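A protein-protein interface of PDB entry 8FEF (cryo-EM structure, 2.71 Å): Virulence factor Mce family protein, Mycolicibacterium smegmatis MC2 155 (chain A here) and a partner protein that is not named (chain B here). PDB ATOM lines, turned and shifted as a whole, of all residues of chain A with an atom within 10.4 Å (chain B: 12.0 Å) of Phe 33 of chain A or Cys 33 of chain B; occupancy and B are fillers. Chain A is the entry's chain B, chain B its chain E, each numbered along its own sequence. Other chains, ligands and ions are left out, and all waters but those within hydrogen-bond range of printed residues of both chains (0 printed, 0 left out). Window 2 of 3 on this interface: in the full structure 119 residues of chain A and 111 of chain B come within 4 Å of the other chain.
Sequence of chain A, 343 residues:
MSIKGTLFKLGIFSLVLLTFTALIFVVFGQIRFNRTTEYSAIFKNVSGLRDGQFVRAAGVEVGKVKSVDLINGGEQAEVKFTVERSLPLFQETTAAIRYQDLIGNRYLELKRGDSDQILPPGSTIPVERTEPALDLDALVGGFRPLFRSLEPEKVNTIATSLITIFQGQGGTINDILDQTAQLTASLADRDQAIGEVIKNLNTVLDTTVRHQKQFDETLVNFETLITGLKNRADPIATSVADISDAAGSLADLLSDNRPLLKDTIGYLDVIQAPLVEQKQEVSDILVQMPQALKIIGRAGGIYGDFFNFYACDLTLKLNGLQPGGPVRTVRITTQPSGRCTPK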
ATOM      1  N   THR A  19      -2.122 -22.286 -31.813  1.00  0.00           N
ATOM      2  CA  THR A  19      -2.335 -23.086 -30.616  1.00  0.00           C
ATOM      3  C   THR A  19      -1.000 -23.505 -30.022  1.00  0.00           C
ATOM      4  O   THR A  19      -0.821 -23.492 -28.800  1.00  0.00           O
ATOM      5  CB  THR A  19      -3.197 -24.306 -30.941  1.00  0.00           C
ATOM      6  OG1 THR A  19      -4.483 -23.872 -31.399  1.00  0.00           O
ATOM      7  CG2 THR A  19      -3.377 -25.184 -29.714  1.00  0.00           C
ATOM      8  N   ALA A  22       0.547 -20.339 -28.367  1.00  0.00           N
ATOM      9  CA  ALA A  22      -0.155 -20.088 -27.113  1.00  0.00           C
ATOM     10  C   ALA A  22       0.217 -21.117 -26.055  1.00  0.00           C
ATOM     11  O   ALA A  22       0.339 -20.782 -24.872  1.00  0.00           O
ATOM     12  CB  ALA A  22      -1.665 -20.080 -27.349  1.00  0.00           C
ATOM     13  N   LEU A  23       0.383 -22.378 -26.457  1.00  0.00           N
ATOM     14  CA  LEU A  23       0.795 -23.413 -25.519  1.00  0.00           C
ATOM     15  C   LEU A  23       2.189 -23.134 -24.976  1.00  0.00           C
ATOM     16  O   LEU A  23       2.451 -23.344 -23.788  1.00  0.00           O
ATOM     17  CB  LEU A  23       0.735 -24.781 -26.202  1.00  0.00           C
ATOM     18  CG  LEU A  23       1.169 -26.031 -25.436  1.00  0.00           C
ATOM     19  CD1 LEU A  23       0.228 -27.174 -25.756  1.00  0.00           C
ATOM     20  CD2 LEU A  23       2.594 -26.419 -25.791  1.00  0.00           C
ATOM     21  N   ILE A  24       3.096 -22.661 -25.833  1.00  0.00           N
ATOM     22  CA  ILE A  24       4.432 -22.294 -25.366  1.00  0.00           C
ATOM     23  C   ILE A  24       4.348 -21.153 -24.360  1.00  0.00           C
ATOM     24  O   ILE A  24       5.018 -21.172 -23.317  1.00  0.00           O
ATOM     25  CB  ILE A  24       5.333 -21.923 -26.558  1.00  0.00           C
ATOM     26  CG1 ILE A  24       5.642 -23.153 -27.404  1.00  0.00           C
ATOM     27  CG2 ILE A  24       6.624 -21.273 -26.084  1.00  0.00           C
ATOM     28  CD1 ILE A  24       6.347 -22.815 -28.680  1.00  0.00           C
ATOM     29  N   PHE A  25       3.522 -20.145 -24.656  1.00  0.00           N
ATOM     30  CA  PHE A  25       3.359 -19.028 -23.726  1.00  0.00           C
ATOM     31  C   PHE A  25       2.780 -19.486 -22.391  1.00  0.00           C
ATOM     32  O   PHE A  25       3.225 -19.035 -21.330  1.00  0.00           O
ATOM     33  CB  PHE A  25       2.479 -17.943 -24.346  1.00  0.00           C
ATOM     34  CG  PHE A  25       3.244 -16.922 -25.137  1.00  0.00           C
ATOM     35  CD1 PHE A  25       3.926 -15.902 -24.495  1.00  0.00           C
ATOM     36  CD2 PHE A  25       3.281 -16.978 -26.518  1.00  0.00           C
ATOM     37  CE1 PHE A  25       4.631 -14.959 -25.217  1.00  0.00           C
ATOM     38  CE2 PHE A  25       3.985 -16.038 -27.245  1.00  0.00           C
ATOM     39  CZ  PHE A  25       4.660 -15.027 -26.593  1.00  0.00           C
ATOM     40  N   VAL A  26       1.793 -20.382 -22.423  1.00  0.00           N
ATOM     41  CA  VAL A  26       1.196 -20.892 -21.191  1.00  0.00           C
ATOM     42  C   VAL A  26       2.213 -21.699 -20.391  1.00  0.00           C
ATOM     43  O   VAL A  26       2.304 -21.564 -19.165  1.00  0.00           O
ATOM     44  CB  VAL A  26      -0.064 -21.717 -21.511  1.00  0.00           C
ATOM     45  CG1 VAL A  26      -0.526 -22.493 -20.293  1.00  0.00           C
ATOM     46  CG2 VAL A  26      -1.176 -20.809 -22.003  1.00  0.00           C
ATOM     47  N   VAL A  27       2.996 -22.542 -21.066  1.00  0.00           N
ATOM     48  CA  VAL A  27       3.927 -23.421 -20.366  1.00  0.00           C
ATOM     49  C   VAL A  27       5.055 -22.618 -19.730  1.00  0.00           C
ATOM     50  O   VAL A  27       5.392 -22.817 -18.558  1.00  0.00           O
ATOM     51  CB  VAL A  27       4.467 -24.501 -21.322  1.00  0.00           C
ATOM     52  CG1 VAL A  27       5.700 -25.161 -20.739  1.00  0.00           C
ATOM     53  CG2 VAL A  27       3.398 -25.544 -21.590  1.00  0.00           C
ATOM     54  N   PHE A  28       5.649 -21.692 -20.478  1.00  0.00           N
ATOM     55  CA  PHE A  28       6.803 -20.968 -19.962  1.00  0.00           C
ATOM     56  C   PHE A  28       6.440 -19.680 -19.239  1.00  0.00           C
ATOM     57  O   PHE A  28       7.330 -19.030 -18.686  1.00  0.00           O
ATOM     58  CB  PHE A  28       7.793 -20.679 -21.091  1.00  0.00           C
ATOM     59  CG  PHE A  28       8.465 -21.908 -21.617  1.00  0.00           C
ATOM     60  CD1 PHE A  28       9.482 -22.509 -20.897  1.00  0.00           C
ATOM     61  CD2 PHE A  28       8.072 -22.474 -22.814  1.00  0.00           C
ATOM     62  CE1 PHE A  28      10.101 -23.643 -21.365  1.00  0.00           C
ATOM     63  CE2 PHE A  28       8.688 -23.610 -23.286  1.00  0.00           C
ATOM     64  CZ  PHE A  28       9.705 -24.195 -22.558  1.00  0.00           C
ATOM     65  N   GLY A  29       5.168 -19.298 -19.218  1.00  0.00           N
ATOM     66  CA  GLY A  29       4.736 -18.131 -18.488  1.00  0.00           C
ATOM     67  C   GLY A  29       4.039 -18.440 -17.188  1.00  0.00           C
ATOM     68  O   GLY A  29       3.709 -17.512 -16.445  1.00  0.00           O
ATOM     69  N   GLN A  30       3.805 -19.721 -16.898  1.00  0.00           N
ATOM     70  CA  GLN A  30       3.150 -20.181 -15.674  1.00  0.00           C
ATOM     71  C   GLN A  30       1.763 -19.551 -15.523  1.00  0.00           C
ATOM     72  O   GLN A  30       1.477 -18.821 -14.574  1.00  0.00           O
ATOM     73  CB  GLN A  30       4.030 -19.902 -14.450  1.00  0.00           C
ATOM     74  CG  GLN A  30       5.416 -20.537 -14.505  1.00  0.00           C
ATOM     75  CD  GLN A  30       5.417 -22.008 -14.139  1.00  0.00           C
ATOM     76  OE1 GLN A  30       4.366 -22.635 -14.013  1.00  0.00           O
ATOM     77  NE2 GLN A  30       6.605 -22.567 -13.961  1.00  0.00           N
ATOM     78  N   ILE A  31       0.901 -19.847 -16.489  1.00  0.00           N
ATOM     79  CA  ILE A  31      -0.453 -19.310 -16.536  1.00  0.00           C
ATOM     80  C   ILE A  31      -1.402 -20.328 -15.921  1.00  0.00           C
ATOM     81  O   ILE A  31      -1.384 -21.507 -16.296  1.00  0.00           O
ATOM     82  CB  ILE A  31      -0.869 -18.970 -17.977  1.00  0.00           C
ATOM     83  CG1 ILE A  31       0.175 -18.071 -18.640  1.00  0.00           C
ATOM     84  CG2 ILE A  31      -2.226 -18.296 -17.997  1.00  0.00           C
ATOM     85  CD1 ILE A  31       0.343 -16.733 -17.973  1.00  0.00           C
ATOM     86  N   ARG A  32      -2.227 -19.882 -14.976  1.00  0.00           N
ATOM     87  CA  ARG A  32      -3.248 -20.724 -14.371  1.00  0.00           C
ATOM     88  C   ARG A  32      -4.626 -20.134 -14.633  1.00  0.00           C
ATOM     89  O   ARG A  32      -4.784 -18.917 -14.761  1.00  0.00           O
ATOM     90  CB  ARG A  32      -3.031 -20.896 -12.863  1.00  0.00           C
ATOM     91  CG  ARG A  32      -2.184 -22.106 -12.492  1.00  0.00           C
ATOM     92  CD  ARG A  32      -0.713 -21.847 -12.733  1.00  0.00           C
ATOM     93  NE  ARG A  32       0.071 -23.074 -12.746  1.00  0.00           N
ATOM     94  CZ  ARG A  32       1.394 -23.109 -12.809  1.00  0.00           C
ATOM     95  NH1 ARG A  32       2.112 -22.000 -12.840  1.00  0.00           N
ATOM     96  NH2 ARG A  32       2.014 -24.284 -12.836  1.00  0.00           N
ATOM     97  N   PHE A  33      -5.623 -21.010 -14.711  1.00  0.00           N
ATOM     98  CA  PHE A  33      -6.987 -20.639 -15.064  1.00  0.00           C
ATOM     99  C   PHE A  33      -7.974 -21.054 -13.981  1.00  0.00           C
ATOM    100  O   PHE A  33      -9.060 -21.560 -14.267  1.00  0.00           O
ATOM    101  CB  PHE A  33      -7.386 -21.251 -16.405  1.00  0.00           C
ATOM    102  CG  PHE A  33      -6.338 -21.115 -17.472  1.00  0.00           C
ATOM    103  CD1 PHE A  33      -6.238 -19.954 -18.219  1.00  0.00           C
ATOM    104  CD2 PHE A  33      -5.458 -22.152 -17.734  1.00  0.00           C
ATOM    105  CE1 PHE A  33      -5.275 -19.829 -19.201  1.00  0.00           C
ATOM    106  CE2 PHE A  33      -4.495 -22.030 -18.712  1.00  0.00           C
ATOM    107  CZ  PHE A  33      -4.403 -20.868 -19.447  1.00  0.00           C
ATOM    108  N   ASN A  34      -7.612 -20.847 -12.717  1.00  0.00           N
ATOM    109  CA  ASN A  34      -8.462 -21.212 -11.596  1.00  0.00           C
ATOM    110  C   ASN A  34      -8.883 -19.967 -10.827  1.00  0.00           C
ATOM    111  O   ASN A  34      -8.153 -18.974 -10.774  1.00  0.00           O
ATOM    112  CB  ASN A  34      -7.751 -22.191 -10.653  1.00  0.00           C
ATOM    113  CG  ASN A  34      -6.504 -21.598 -10.027  1.00  0.00           C
ATOM    114  OD1 ASN A  34      -5.857 -20.728 -10.609  1.00  0.00           O
ATOM    115  ND2 ASN A  34      -6.159 -22.068  -8.836  1.00  0.00           N
ATOM    116  N   ARG A  35     -10.075 -20.029 -10.239  1.00  0.00           N
ATOM    117  CA  ARG A  35     -10.568 -18.932  -9.419  1.00  0.00           C
ATOM    118  C   ARG A  35      -9.810 -18.890  -8.098  1.00  0.00           C
ATOM    119  O   ARG A  35      -9.633 -19.919  -7.440  1.00  0.00           O
ATOM    120  CB  ARG A  35     -12.070 -19.083  -9.180  1.00  0.00           C
ATOM    121  CG  ARG A  35     -12.902 -18.799 -10.422  1.00  0.00           C
ATOM    122  CD  ARG A  35     -14.301 -19.395 -10.349  1.00  0.00           C
ATOM    123  NE  ARG A  35     -15.118 -18.809  -9.293  1.00  0.00           N
ATOM    124  CZ  ARG A  35     -15.590 -19.479  -8.251  1.00  0.00           C
ATOM    125  NH1 ARG A  35     -15.344 -20.769  -8.091  1.00  0.00           N
ATOM    126  NH2 ARG A  35     -16.334 -18.842  -7.352  1.00  0.00           N
ATOM    127  N   THR A  36      -9.358 -17.698  -7.712  1.00  0.00           N
ATOM    128  CA  THR A  36      -8.484 -17.533  -6.561  1.00  0.00           C
ATOM    129  C   THR A  36      -9.009 -16.430  -5.652  1.00  0.00           C
ATOM    130  O   THR A  36      -9.750 -15.541  -6.074  1.00  0.00           O
ATOM    131  CB  THR A  36      -7.044 -17.203  -6.987  1.00  0.00           C
ATOM    132  OG1 THR A  36      -7.054 -16.097  -7.897  1.00  0.00           O
ATOM    133  CG2 THR A  36      -6.390 -18.400  -7.656  1.00  0.00           C
ATOM    134  N   GLU A  61       0.804 -26.892  -4.439  1.00  0.00           N
ATOM    135  CA  GLU A  61       0.576 -25.581  -5.040  1.00  0.00           C
ATOM    136  C   GLU A  61      -0.906 -25.228  -5.058  1.00  0.00           C
ATOM    137  O   GLU A  61      -1.740 -26.010  -5.522  1.00  0.00           O
ATOM    138  CB  GLU A  61       1.136 -25.556  -6.460  1.00  0.00           C
ATOM    139  CG  GLU A  61       0.735 -24.331  -7.259  1.00  0.00           C
ATOM    140  CD  GLU A  61       1.029 -24.477  -8.737  1.00  0.00           C
ATOM    141  OE1 GLU A  61       1.761 -25.418  -9.107  1.00  0.00           O
ATOM    142  OE2 GLU A  61       0.525 -23.654  -9.528  1.00  0.00           O
ATOM    143  N   VAL A  62      -1.231 -24.036  -4.553  1.00  0.00           N
ATOM    144  CA  VAL A  62      -2.620 -23.597  -4.452  1.00  0.00           C
ATOM    145  C   VAL A  62      -2.786 -22.182  -4.995  1.00  0.00           C
ATOM    146  O   VAL A  62      -3.915 -21.718  -5.190  1.00  0.00           O
ATOM    147  CB  VAL A  62      -3.130 -23.685  -3.000  1.00  0.00           C
ATOM    148  CG1 VAL A  62      -3.286 -25.134  -2.572  1.00  0.00           C
ATOM    149  CG2 VAL A  62      -2.199 -22.944  -2.060  1.00  0.00           C
ATOM    150  N   GLY A  63      -1.688 -21.483  -5.240  1.00  0.00           N
ATOM    151  CA  GLY A  63      -1.807 -20.144  -5.774  1.00  0.00           C
ATOM    152  C   GLY A  63      -0.475 -19.538  -6.145  1.00  0.00           C
ATOM    153  O   GLY A  63       0.535 -20.231  -6.249  1.00  0.00           O
ATOM    154  N   LYS A  64      -0.485 -18.222  -6.336  1.00  0.00           N
ATOM    155  CA  LYS A  64       0.703 -17.471  -6.716  1.00  0.00           C
ATOM    156  C   LYS A  64       0.868 -16.255  -5.817  1.00  0.00           C
ATOM    157  O   LYS A  64      -0.042 -15.864  -5.081  1.00  0.00           O
ATOM    158  CB  LYS A  64       0.643 -17.021  -8.179  1.00  0.00           C
ATOM    159  CG  LYS A  64       1.050 -18.077  -9.177  1.00  0.00           C
ATOM    160  CD  LYS A  64       1.244 -17.450 -10.536  1.00  0.00           C
ATOM    161  CE  LYS A  64       2.025 -18.354 -11.454  1.00  0.00           C
ATOM    162  NZ  LYS A  64       2.378 -17.637 -12.707  1.00  0.00           N
ATOM    163  N   THR A  82      -2.294 -15.165  -3.681  1.00  0.00           N
ATOM    164  CA  THR A  82      -3.567 -15.790  -4.003  1.00  0.00           C
ATOM    165  C   THR A  82      -3.559 -17.249  -3.571  1.00  0.00           C
ATOM    166  O   THR A  82      -2.516 -17.907  -3.556  1.00  0.00           O
ATOM    167  CB  THR A  82      -3.884 -15.708  -5.500  1.00  0.00           C
ATOM    168  OG1 THR A  82      -2.824 -16.311  -6.252  1.00  0.00           O
ATOM    169  CG2 THR A  82      -4.053 -14.264  -5.932  1.00  0.00           C
ATOM    170  N   GLU A  84      -6.147 -20.901  -3.947  1.00  0.00           N
ATOM    171  CA  GLU A  84      -7.285 -21.513  -4.623  1.00  0.00           C
ATOM    172  C   GLU A  84      -8.561 -21.331  -3.808  1.00  0.00           C
ATOM    173  O   GLU A  84      -8.576 -21.571  -2.597  1.00  0.00           O
ATOM    174  CB  GLU A  84      -7.011 -22.999  -4.859  1.00  0.00           C
ATOM    175  CG  GLU A  84      -8.094 -23.718  -5.636  1.00  0.00           C
ATOM    176  CD  GLU A  84      -7.777 -25.185  -5.846  1.00  0.00           C
ATOM    177  OE1 GLU A  84      -6.743 -25.651  -5.324  1.00  0.00           O
ATOM    178  OE2 GLU A  84      -8.560 -25.873  -6.532  1.00  0.00           O
ATOM    179  N   ARG A  85      -9.626 -20.889  -4.481  1.00  0.00           N
ATOM    180  CA  ARG A  85     -10.852 -20.501  -3.787  1.00  0.00           C
ATOM    181  C   ARG A  85     -11.477 -21.665  -3.028  1.00  0.00           C
ATOM    182  O   ARG A  85     -12.175 -21.452  -2.029  1.00  0.00           O
ATOM    183  CB  ARG A  85     -11.848 -19.916  -4.789  1.00  0.00           C
ATOM    184  CG  ARG A  85     -13.091 -19.309  -4.168  1.00  0.00           C
ATOM    185  CD  ARG A  85     -13.821 -18.421  -5.158  1.00  0.00           C
ATOM    186  NE  ARG A  85     -12.995 -17.298  -5.584  1.00  0.00           N
ATOM    187  CZ  ARG A  85     -13.391 -16.350  -6.422  1.00  0.00           C
ATOM    188  NH1 ARG A  85     -14.606 -16.353  -6.945  1.00  0.00           N
ATOM    189  NH2 ARG A  85     -12.548 -15.374  -6.742  1.00  0.00           N
ATOM    190  N   CYS B  33      -7.825 -27.695 -18.050  1.00  0.00           N
ATOM    191  CA  CYS B  33      -7.909 -26.239 -18.058  1.00  0.00           C
ATOM    192  C   CYS B  33      -8.090 -25.695 -16.646  1.00  0.00           C
ATOM    193  O   CYS B  33      -7.273 -24.912 -16.163  1.00  0.00           O
ATOM    194  CB  CYS B  33      -9.058 -25.774 -18.954  1.00  0.00           C
ATOM    195  SG  CYS B  33      -9.204 -23.980 -19.113  1.00  0.00           S
ATOM    196  N   GLY B  34      -9.176 -26.110 -15.992  1.00  0.00           N
ATOM    197  CA  GLY B  34      -9.419 -25.671 -14.627  1.00  0.00           C
ATOM    198  C   GLY B  34      -8.405 -26.219 -13.641  1.00  0.00           C
ATOM    199  O   GLY B  34      -8.002 -25.527 -12.701  1.00  0.00           O
ATOM    200  N   GLN B  35      -7.979 -27.466 -13.837  1.00  0.00           N
ATOM    201  CA  GLN B  35      -7.042 -28.125 -12.939  1.00  0.00           C
ATOM    202  C   GLN B  35      -5.601 -28.044 -13.423  1.00  0.00           C
ATOM    203  O   GLN B  35      -4.734 -28.719 -12.860  1.00  0.00           O
ATOM    204  CB  GLN B  35      -7.438 -29.590 -12.746  1.00  0.00           C
ATOM    205  CG  GLN B  35      -7.275 -30.443 -13.994  1.00  0.00           C
ATOM    206  CD  GLN B  35      -7.548 -31.912 -13.740  1.00  0.00           C
ATOM    207  OE1 GLN B  35      -8.042 -32.288 -12.677  1.00  0.00           O
ATOM    208  NE2 GLN B  35      -7.223 -32.751 -14.715  1.00  0.00           N
ATOM    209  N   TRP B  36      -5.329 -27.246 -14.458  1.00  0.00           N
ATOM    210  CA  TRP B  36      -3.986 -27.130 -15.014  1.00  0.00           C
ATOM    211  C   TRP B  36      -3.009 -26.605 -13.970  1.00  0.00           C
ATOM    212  O   TRP B  36      -3.117 -25.456 -13.533  1.00  0.00           O
ATOM    213  CB  TRP B  36      -3.996 -26.217 -16.241  1.00  0.00           C
ATOM    214  CG  TRP B  36      -2.634 -25.883 -16.764  1.00  0.00           C
ATOM    215  CD1 TRP B  36      -1.940 -24.727 -16.562  1.00  0.00           C
ATOM    216  CD2 TRP B  36      -1.803 -26.714 -17.580  1.00  0.00           C
ATOM    217  NE1 TRP B  36      -0.726 -24.788 -17.199  1.00  0.00           N
ATOM    218  CE2 TRP B  36      -0.617 -25.998 -17.832  1.00  0.00           C
ATOM    219  CE3 TRP B  36      -1.944 -27.995 -18.121  1.00  0.00           C
ATOM    220  CZ2 TRP B  36       0.418 -26.517 -18.602  1.00  0.00           C
ATOM    221  CZ3 TRP B  36      -0.915 -28.509 -18.882  1.00  0.00           C
ATOM    222  CH2 TRP B  36       0.251 -27.772 -19.116  1.00  0.00           C
ATOM    223  N   ARG B  37      -2.054 -27.438 -13.567  1.00  0.00           N
ATOM    224  CA  ARG B  37      -1.052 -27.055 -12.586  1.00  0.00           C
ATOM    225  C   ARG B  37       0.332 -26.858 -13.184  1.00  0.00           C
ATOM    226  O   ARG B  37       1.254 -26.471 -12.461  1.00  0.00           O
ATOM    227  CB  ARG B  37      -0.982 -28.096 -11.463  1.00  0.00           C
ATOM    228  CG  ARG B  37      -1.335 -27.536 -10.099  1.00  0.00           C
ATOM    229  CD  ARG B  37      -2.747 -26.985 -10.096  1.00  0.00           C
ATOM    230  NE  ARG B  37      -2.901 -25.878  -9.160  1.00  0.00           N
ATOM    231  CZ  ARG B  37      -4.036 -25.225  -8.955  1.00  0.00           C
ATOM    232  NH1 ARG B  37      -5.146 -25.552  -9.596  1.00  0.00           N
ATOM    233  NH2 ARG B  37      -4.060 -24.222  -8.083  1.00  0.00           N
ATOM    234  N   GLY B  38       0.508 -27.113 -14.474  1.00  0.00           N
ATOM    235  CA  GLY B  38       1.779 -26.900 -15.133  1.00  0.00           C
ATOM    236  C   GLY B  38       2.194 -28.101 -15.958  1.00  0.00           C
ATOM    237  O   GLY B  38       1.610 -29.180 -15.887  1.00  0.00           O
ATOM    238  N   ILE B  39       3.236 -27.881 -16.762  1.00  0.00           N
ATOM    239  CA  ILE B  39       3.800 -28.968 -17.549  1.00  0.00           C
ATOM    240  C   ILE B  39       4.557 -29.947 -16.659  1.00  0.00           C
ATOM    241  O   ILE B  39       4.757 -31.106 -17.041  1.00  0.00           O
ATOM    242  CB  ILE B  39       4.700 -28.397 -18.666  1.00  0.00           C
ATOM    243  CG1 ILE B  39       5.043 -29.471 -19.702  1.00  0.00           C
ATOM    244  CG2 ILE B  39       5.966 -27.786 -18.083  1.00  0.00           C
ATOM    245  CD1 ILE B  39       3.836 -30.080 -20.371  1.00  0.00           C
ATOM    246  N   ASN B  41       3.415 -30.989 -13.739  1.00  0.00           N
ATOM    247  CA  ASN B  41       2.442 -31.705 -12.925  1.00  0.00           C
ATOM    248  C   ASN B  41       1.451 -32.501 -13.767  1.00  0.00           C
ATOM    249  O   ASN B  41       0.361 -32.830 -13.289  1.00  0.00           O
ATOM    250  CB  ASN B  41       1.700 -30.729 -12.012  1.00  0.00           C
ATOM    251  CG  ASN B  41       2.601 -30.125 -10.954  1.00  0.00           C
ATOM    252  OD1 ASN B  41       3.290 -30.838 -10.228  1.00  0.00           O
ATOM    253  ND2 ASN B  41       2.603 -28.800 -10.867  1.00  0.00           N
ATOM    254  N   VAL B  42       1.804 -32.812 -15.010  1.00  0.00           N
ATOM    255  CA  VAL B  42       0.957 -33.630 -15.875  1.00  0.00           C
ATOM    256  C   VAL B  42       1.562 -35.027 -15.968  1.00  0.00           C
ATOM    257  O   VAL B  42       2.790 -35.163 -16.067  1.00  0.00           O
ATOM    258  CB  VAL B  42       0.777 -32.967 -17.256  1.00  0.00           C
ATOM    259  CG1 VAL B  42       2.100 -32.836 -17.994  1.00  0.00           C
ATOM    260  CG2 VAL B  42      -0.229 -33.731 -18.102  1.00  0.00           C
ATOM    261  N   PRO B  43       0.761 -36.088 -15.851  1.00  0.00           N
ATOM    262  CA  PRO B  43       1.312 -37.444 -15.970  1.00  0.00           C
ATOM    263  C   PRO B  43       1.949 -37.671 -17.333  1.00  0.00           C
ATOM    264  O   PRO B  43       1.445 -37.216 -18.361  1.00  0.00           O
ATOM    265  CB  PRO B  43       0.089 -38.344 -15.760  1.00  0.00           C
ATOM    266  CG  PRO B  43      -0.868 -37.505 -14.996  1.00  0.00           C
ATOM    267  CD  PRO B  43      -0.666 -36.107 -15.487  1.00  0.00           C
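The backbone carbonyl oxygen (O) of Val 62 of chain A lies within hydrogen-bond range of the backbone NH (N) of Glu 84 of chain A.
O of Val 26 of chain A is in hydrogen-bond range of N of Ile 31 of chain A, at 3.5 Å.
OE1 of Gln 30 of chain A lies within hydrogen-bond range of NH1 of Arg 32 of chain A.
The side-chain amide nitrogen (ND2) of Asn 41 of chain B lies within hydrogen-bond range of the backbone carbonyl oxygen (O) of Arg 37 of chain B (3.1 Å).
NE of Arg 32 of chain A lies within salt-bridge range of OE2 of Glu 61 of chain A.
NH2 of Arg 37 of chain B sits close to ND2 of Asn 34 of chain A, at 3.1 Å.
O of Ile 31 of chain A lies close to NE1 of Trp 36 of chain B (3.5 Å).
The guanidinium group of Arg 32 of chain A lies close to the backbone carbonyl oxygen of Arg 37 of chain B (2.3 Å).
Trp 36 of chain B touches Val 26 of chain A.
CG2 of Ile 39 of chain B touches CG1 of Val 27 of chain A, 3.7 Å away.
Arg 32 of chain A touches Trp 36 of chain B.
NH2 of Arg 32 of chain A touches CA of Gly 38 of chain B, at 3.5 Å.
Phe 33 of chain A touches Cys 33 of chain B (CD2 to O, 3.7 Å).
CB of Asn 34 of chain A touches O of Gly 34 of chain B (3.9 Å).
OE1 of Glu 61 of chain A touches O of Arg 37 of chain B, at 3.6 Å.
Glu 61 of chain A touches Asn 41 of chain B.
O of Val 62 of chain A touches NH2 of Arg 37 of chain B, at 3.8 Å.
Thr 19 of chain A touches none of the printed residues of chain B.
Of chain B, only Trp 36 (3.9 Å) comes within 4 Å of Val 26 of chain A.
Of chain B, only Trp 36 (3.3 Å) comes within 4 Å of Ile 31 of chain A.
Of chain B, only Cys 33 comes within 4 Å of Phe 33 of chain A.
Of the printed residues of chain B, Val 62 of chain A touches Arg 37.
Of chain A, only Phe 33 comes within 4 Å of Cys 33 of chain B.
Of chain A, only Asn 34 (3.9 Å) comes within 4 Å of Gly 34 of chain B.
Of the printed residues of chain A, Gly 38 of chain B touches Arg 32 (3.5 Å).
Of the printed residues of chain A, Ile 39 of chain B touches Val 27 (3.7 Å).
The nearest residue of chain B that does not touch Phe 33 of chain A is Gly 34 of chain B (4.1 Å).
The nearest residue of chain A that does not touch Cys 33 of chain B is Asn 34 of chain A (5.3 Å).
The nearest printed residue of chain A that does not touch Arg 37 of chain B is Glu 84 of chain A (4.1 Å).
Of the 10 printed residues of chain B, 7 touch a printed residue of chain A.
Hydrophobic or aromatic side chains of chain B within 4 Å of the printed part of chain A: Trp 36 and Ile 39.
Of the 23 printed residues of chain A, 8 touch a printed residue of chain B.
Hydrophobic or aromatic side chains of chain A within 4 Å of the printed part of chain B: Val 26, Val 27 and Phe 33.
Among the printed residues, no Asp or Glu carboxylate lies within 4 Å of a Lys or Arg side-chain nitrogen of the other chain.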
